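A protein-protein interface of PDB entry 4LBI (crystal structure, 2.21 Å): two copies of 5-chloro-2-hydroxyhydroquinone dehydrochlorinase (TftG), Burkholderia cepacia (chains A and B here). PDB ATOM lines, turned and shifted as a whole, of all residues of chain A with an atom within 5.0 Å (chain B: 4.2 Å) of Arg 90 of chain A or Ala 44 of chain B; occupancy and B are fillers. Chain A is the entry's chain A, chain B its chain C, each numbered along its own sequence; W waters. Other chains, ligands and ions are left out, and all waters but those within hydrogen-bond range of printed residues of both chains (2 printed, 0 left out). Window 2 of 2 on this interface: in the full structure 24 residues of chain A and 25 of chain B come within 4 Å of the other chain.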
ATOM      1  N   MET A   1     -11.384 -20.375 -15.495  1.00  0.00           N
ATOM      2  CA  MET A   1     -10.426 -19.816 -16.441  1.00  0.00           C
ATOM      3  C   MET A   1      -9.020 -20.098 -15.946  1.00  0.00           C
ATOM      4  O   MET A   1      -8.785 -20.079 -14.738  1.00  0.00           O
ATOM      5  CB  MET A   1     -10.607 -18.302 -16.569  1.00  0.00           C
ATOM      6  CG  MET A   1     -11.698 -17.853 -17.522  1.00  0.00           C
ATOM      7  SD  MET A   1     -11.741 -15.891 -17.673  1.00  0.00           S
ATOM      8  CE  MET A   1     -12.706 -15.584 -16.091  1.00  0.00           C
ATOM      9  N   LEU A   2      -8.090 -20.344 -16.874  1.00  0.00           N
ATOM     10  CA  LEU A   2      -6.679 -20.487 -16.530  1.00  0.00           C
ATOM     11  C   LEU A   2      -5.869 -19.216 -16.825  1.00  0.00           C
ATOM     12  O   LEU A   2      -6.090 -18.549 -17.842  1.00  0.00           O
ATOM     13  CB  LEU A   2      -6.072 -21.685 -17.258  1.00  0.00           C
ATOM     14  CG  LEU A   2      -6.748 -23.017 -16.917  1.00  0.00           C
ATOM     15  CD1 LEU A   2      -6.076 -24.175 -17.645  1.00  0.00           C
ATOM     16  CD2 LEU A   2      -6.755 -23.249 -15.400  1.00  0.00           C
ATOM     17  N   PHE A   3      -4.934 -18.889 -15.931  1.00  0.00           N
ATOM     18  CA  PHE A   3      -4.073 -17.728 -16.110  1.00  0.00           C
ATOM     19  C   PHE A   3      -2.593 -18.040 -15.913  1.00  0.00           C
ATOM     20  O   PHE A   3      -2.199 -18.704 -14.950  1.00  0.00           O
ATOM     21  CB  PHE A   3      -4.465 -16.596 -15.154  1.00  0.00           C
ATOM     22  CG  PHE A   3      -5.823 -16.007 -15.425  1.00  0.00           C
ATOM     23  CD1 PHE A   3      -5.960 -14.890 -16.238  1.00  0.00           C
ATOM     24  CD2 PHE A   3      -6.958 -16.566 -14.869  1.00  0.00           C
ATOM     25  CE1 PHE A   3      -7.211 -14.336 -16.486  1.00  0.00           C
ATOM     26  CE2 PHE A   3      -8.213 -16.025 -15.111  1.00  0.00           C
ATOM     27  CZ  PHE A   3      -8.340 -14.911 -15.919  1.00  0.00           C
ATOM     28  N   TRP A  65     -10.697 -12.144 -14.090  1.00  0.00           N
ATOM     29  CA  TRP A  65      -9.489 -11.333 -13.985  1.00  0.00           C
ATOM     30  C   TRP A  65      -9.414 -10.674 -12.614  1.00  0.00           C
ATOM     31  O   TRP A  65      -8.342 -10.609 -12.003  1.00  0.00           O
ATOM     32  CB  TRP A  65      -9.420 -10.263 -15.081  1.00  0.00           C
ATOM     33  CG  TRP A  65      -8.963 -10.786 -16.421  1.00  0.00           C
ATOM     34  CD1 TRP A  65      -9.735 -11.411 -17.361  1.00  0.00           C
ATOM     35  CD2 TRP A  65      -7.639 -10.710 -16.977  1.00  0.00           C
ATOM     36  NE1 TRP A  65      -8.974 -11.738 -18.460  1.00  0.00           N
ATOM     37  CE2 TRP A  65      -7.686 -11.318 -18.253  1.00  0.00           C
ATOM     38  CE3 TRP A  65      -6.422 -10.188 -16.524  1.00  0.00           C
ATOM     39  CZ2 TRP A  65      -6.556 -11.418 -19.083  1.00  0.00           C
ATOM     40  CZ3 TRP A  65      -5.301 -10.282 -17.353  1.00  0.00           C
ATOM     41  CH2 TRP A  65      -5.377 -10.903 -18.611  1.00  0.00           C
ATOM     42  N   VAL A  88       0.092 -11.014 -16.603  1.00  0.00           N
ATOM     43  CA  VAL A  88      -0.991 -11.972 -16.446  1.00  0.00           C
ATOM     44  C   VAL A  88      -1.600 -12.220 -17.827  1.00  0.00           C
ATOM     45  O   VAL A  88      -1.787 -11.279 -18.600  1.00  0.00           O
ATOM     46  CB  VAL A  88      -2.071 -11.432 -15.468  1.00  0.00           C
ATOM     47  CG1 VAL A  88      -3.305 -12.353 -15.420  1.00  0.00           C
ATOM     48  CG2 VAL A  88      -1.475 -11.227 -14.068  1.00  0.00           C
ATOM     49  N   GLU A  89      -1.891 -13.479 -18.142  1.00  0.00           N
ATOM     50  CA  GLU A  89      -2.464 -13.838 -19.431  1.00  0.00           C
ATOM     51  C   GLU A  89      -3.489 -14.950 -19.273  1.00  0.00           C
ATOM     52  O   GLU A  89      -3.197 -15.981 -18.671  1.00  0.00           O
ATOM     53  CB  GLU A  89      -1.375 -14.330 -20.384  1.00  0.00           C
ATOM     54  CG  GLU A  89      -0.367 -13.288 -20.815  1.00  0.00           C
ATOM     55  CD  GLU A  89      -0.846 -12.484 -21.998  1.00  0.00           C
ATOM     56  OE1 GLU A  89      -1.939 -12.793 -22.534  1.00  0.00           O
ATOM     57  OE2 GLU A  89      -0.122 -11.544 -22.395  1.00  0.00           O
ATOM     58  N   ARG A  90      -4.688 -14.739 -19.811  1.00  0.00           N
ATOM     59  CA  ARG A  90      -5.643 -15.827 -19.953  1.00  0.00           C
ATOM     60  C   ARG A  90      -5.002 -16.849 -20.905  1.00  0.00           C
ATOM     61  O   ARG A  90      -4.274 -16.472 -21.825  1.00  0.00           O
ATOM     62  CB  ARG A  90      -6.984 -15.301 -20.484  1.00  0.00           C
ATOM     63  CG  ARG A  90      -8.126 -16.328 -20.465  1.00  0.00           C
ATOM     64  CD  ARG A  90      -9.491 -15.663 -20.700  1.00  0.00           C
ATOM     65  NE  ARG A  90      -9.698 -15.286 -22.095  1.00  0.00           N
ATOM     66  CZ  ARG A  90     -10.286 -16.066 -23.002  1.00  0.00           C
ATOM     67  NH1 ARG A  90     -10.726 -17.273 -22.658  1.00  0.00           N
ATOM     68  NH2 ARG A  90     -10.446 -15.638 -24.252  1.00  0.00           N
ATOM     69  N   TRP A  91      -5.261 -18.134 -20.681  1.00  0.00           N
ATOM     70  CA  TRP A  91      -4.470 -19.191 -21.315  1.00  0.00           C
ATOM     71  C   TRP A  91      -5.215 -20.519 -21.311  1.00  0.00           C
ATOM     72  O   TRP A  91      -6.164 -20.709 -20.538  1.00  0.00           O
ATOM     73  CB  TRP A  91      -3.168 -19.349 -20.532  1.00  0.00           C
ATOM     74  CG  TRP A  91      -2.242 -20.383 -21.052  1.00  0.00           C
ATOM     75  CD1 TRP A  91      -1.361 -20.250 -22.093  1.00  0.00           C
ATOM     76  CD2 TRP A  91      -2.071 -21.712 -20.550  1.00  0.00           C
ATOM     77  NE1 TRP A  91      -0.663 -21.418 -22.274  1.00  0.00           N
ATOM     78  CE2 TRP A  91      -1.077 -22.332 -21.339  1.00  0.00           C
ATOM     79  CE3 TRP A  91      -2.662 -22.441 -19.514  1.00  0.00           C
ATOM     80  CZ2 TRP A  91      -0.662 -23.645 -21.122  1.00  0.00           C
ATOM     81  CZ3 TRP A  91      -2.245 -23.750 -19.297  1.00  0.00           C
ATOM     82  CH2 TRP A  91      -1.255 -24.337 -20.097  1.00  0.00           C
ATOM     83  N   LYS A  92      -4.785 -21.442 -22.163  1.00  0.00           N
ATOM     84  CA  LYS A  92      -5.338 -22.795 -22.155  1.00  0.00           C
ATOM     85  C   LYS A  92      -4.287 -23.779 -22.631  1.00  0.00           C
ATOM     86  O   LYS A  92      -3.390 -23.403 -23.394  1.00  0.00           O
ATOM     87  CB  LYS A  92      -6.574 -22.893 -23.057  1.00  0.00           C
ATOM     88  CG  LYS A  92      -6.267 -22.877 -24.538  1.00  0.00           C
ATOM     89  CD  LYS A  92      -7.433 -23.429 -25.353  1.00  0.00           C
ATOM     90  CE  LYS A  92      -7.076 -23.494 -26.832  1.00  0.00           C
ATOM     91  NZ  LYS A  92      -8.176 -24.047 -27.676  1.00  0.00           N
ATOM     92  N   THR B  41      -1.930 -18.329 -25.416  1.00  0.00           N
ATOM     93  CA  THR B  41      -2.541 -17.327 -24.550  1.00  0.00           C
ATOM     94  C   THR B  41      -3.830 -16.916 -25.242  1.00  0.00           C
ATOM     95  O   THR B  41      -3.929 -17.027 -26.469  1.00  0.00           O
ATOM     96  CB  THR B  41      -1.645 -16.079 -24.387  1.00  0.00           C
ATOM     97  OG1 THR B  41      -1.396 -15.515 -25.672  1.00  0.00           O
ATOM     98  CG2 THR B  41      -0.304 -16.430 -23.729  1.00  0.00           C
ATOM     99  N   LEU B  42      -4.811 -16.441 -24.478  1.00  0.00           N
ATOM    100  CA  LEU B  42      -6.112 -16.077 -25.039  1.00  0.00           C
ATOM    101  C   LEU B  42      -6.445 -14.595 -24.882  1.00  0.00           C
ATOM    102  O   LEU B  42      -5.905 -13.909 -24.022  1.00  0.00           O
ATOM    103  CB  LEU B  42      -7.206 -16.929 -24.408  1.00  0.00           C
ATOM    104  CG  LEU B  42      -6.986 -18.409 -24.677  1.00  0.00           C
ATOM    105  CD1 LEU B  42      -7.845 -19.274 -23.761  1.00  0.00           C
ATOM    106  CD2 LEU B  42      -7.276 -18.692 -26.136  1.00  0.00           C
ATOM    107  N   GLY B  43      -7.355 -14.103 -25.713  1.00  0.00           N
ATOM    108  CA  GLY B  43      -7.704 -12.691 -25.701  1.00  0.00           C
ATOM    109  C   GLY B  43      -8.916 -12.339 -24.852  1.00  0.00           C
ATOM    110  O   GLY B  43      -9.177 -12.996 -23.835  1.00  0.00           O
ATOM    111  N   ALA B  44      -9.646 -11.301 -25.275  1.00  0.00           N
ATOM    112  CA  ALA B  44     -10.830 -10.792 -24.567  1.00  0.00           C
ATOM    113  C   ALA B  44     -11.922 -11.837 -24.432  1.00  0.00           C
ATOM    114  O   ALA B  44     -12.097 -12.671 -25.313  1.00  0.00           O
ATOM    115  CB  ALA B  44     -11.389  -9.569 -25.284  1.00  0.00           C
ATOM    116  N   GLY B  45     -12.656 -11.792 -23.326  1.00  0.00           N
ATOM    117  CA  GLY B  45     -13.804 -12.662 -23.158  1.00  0.00           C
ATOM    118  C   GLY B  45     -13.493 -14.027 -22.584  1.00  0.00           C
ATOM    119  O   GLY B  45     -12.513 -14.185 -21.867  1.00  0.00           O
ATOM    120  N   THR B  46     -14.323 -15.016 -22.908  1.00  0.00           N
ATOM    121  CA  THR B  46     -14.227 -16.334 -22.289  1.00  0.00           C
ATOM    122  C   THR B  46     -14.062 -17.457 -23.318  1.00  0.00           C
ATOM    123  O   THR B  46     -13.957 -18.626 -22.956  1.00  0.00           O
ATOM    124  CB  THR B  46     -15.486 -16.630 -21.452  1.00  0.00           C
ATOM    125  OG1 THR B  46     -16.641 -16.563 -22.297  1.00  0.00           O
ATOM    126  CG2 THR B  46     -15.643 -15.614 -20.335  1.00  0.00           C
ATOM    127  N   GLY B  47     -14.047 -17.104 -24.601  1.00  0.00           N
ATOM    128  CA  GLY B  47     -13.880 -18.091 -25.651  1.00  0.00           C
ATOM    129  C   GLY B  47     -12.533 -18.792 -25.587  1.00  0.00           C
ATOM    130  O   GLY B  47     -11.538 -18.200 -25.168  1.00  0.00           O
ATOM    131  N   THR B  48     -12.502 -20.063 -25.974  1.00  0.00           N
ATOM    132  CA  THR B  48     -11.252 -20.814 -25.979  1.00  0.00           C
ATOM    133  C   THR B  48     -11.032 -21.516 -27.312  1.00  0.00           C
ATOM    134  O   THR B  48     -10.454 -22.591 -27.361  1.00  0.00           O
ATOM    135  CB  THR B  48     -11.195 -21.858 -24.850  1.00  0.00           C
ATOM    136  OG1 THR B  48     -12.286 -22.780 -24.990  1.00  0.00           O
ATOM    137  CG2 THR B  48     -11.280 -21.184 -23.500  1.00  0.00           C
HETATM  138  O   HOH W   1     -10.649 -12.391 -20.317  1.00  0.00           O
HETATM  139  O   HOH W   2      -4.821 -12.655 -22.013  1.00  0.00           O
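The backbone carbonyl oxygen of Thr 48 of chain B is in hydrogen-bond range of the side-chain amino group of Lys 92 of chain A.
The backbone carbonyl oxygen (O) of Gly 43 of chain B sits at hydrogen-bond distance from the guanidinium group (NE) of Arg 90 of chain A, at 2.9 Å.
NH1 of Arg 90 of chain A lies within hydrogen-bond range of O of Gly 47 of chain B (2.8 Å).
The backbone NH (N) of Leu 42 of chain B is in hydrogen-bond range of the backbone carbonyl oxygen (O) of Arg 90 of chain A (2.7 Å).
NE of Arg 90 of chain A lies within hydrogen-bond range of O of Gly 45 of chain B (3.0 Å).
O of Leu 2 of chain A lies within hydrogen-bond range of N of Trp 91 of chain A (3.0 Å).
Among the printed residues, pairs that only touch across the chains: Glu 89 of chain A with Thr 41 of chain B (3.8 Å), Arg 90 of chain A with Thr 41 of chain B (3.3 Å), Arg 90 of chain A with Ala 44 of chain B (3.6 Å), Arg 90 of chain A with Thr 46 of chain B (3.4 Å), Trp 91 of chain A with Thr 41 of chain B (3.9 Å), Trp 91 of chain A with Leu 42 of chain B (3.8 Å) and Lys 92 of chain A with Leu 42 of chain B (3.9 Å).
Of the printed residues of chain B, Arg 90 of chain A touches Thr 41 (3.3 Å), Leu 42 (2.7 Å), Gly 43 (2.9 Å), Ala 44 (3.6 Å), Gly 45 (3.0 Å), Thr 46 (3.4 Å) and Gly 47 (2.8 Å).
Ala 44 of chain B touches one residue of chain A.
Of the printed residues of chain A, Gly 45 of chain B touches Arg 90 (3.0 Å).
Of the printed residues of chain A, Thr 46 of chain B touches Arg 90 (3.4 Å).
Of the printed residues of chain A, Gly 47 of chain B touches Arg 90 (2.8 Å).
Val 88 of chain A touches none of the printed residues of chain B.
The nearest printed residue of chain A that does not touch Ala 44 of chain B is Trp 65 of chain A (6.5 Å).
The nearest printed residue of chain A that does not touch Thr 46 of chain B is Met 1 of chain A (4.7 Å).
Of the 8 printed residues of chain B, 8 touch a printed residue of chain A.
Hydrophobic or aromatic side chains of chain B that line the printed part of chain A: Leu 42.
Of the 9 printed residues of chain A, 4 touch a printed residue of chain B.
Hydrophobic or aromatic side chains of chain A within 4 Å of the printed part of chain B: Trp 91.
Among the printed residues, 12 pairs touch across the chains.
Among the printed residues, no Asp or Glu carboxylate lies within 4 Å of a Lys or Arg side-chain nitrogen of the other chain.
No position is printed for both chains.
Of the 12 pairs that touch across the chains among the printed residues, none has its exchanged pair printed and touching as well.
Water W1 bridges the indole nitrogen (NE1) of Trp 65 of chain A and the backbone carbonyl oxygen (O) of Gly 45 of chain B.
Water W2 lies within hydrogen-bond range of O of Leu 42 of chain B (2.6 Å), OE1 of Glu 89 of chain A (2.9 Å) and N of Arg 90 of chain A (3.0 Å).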
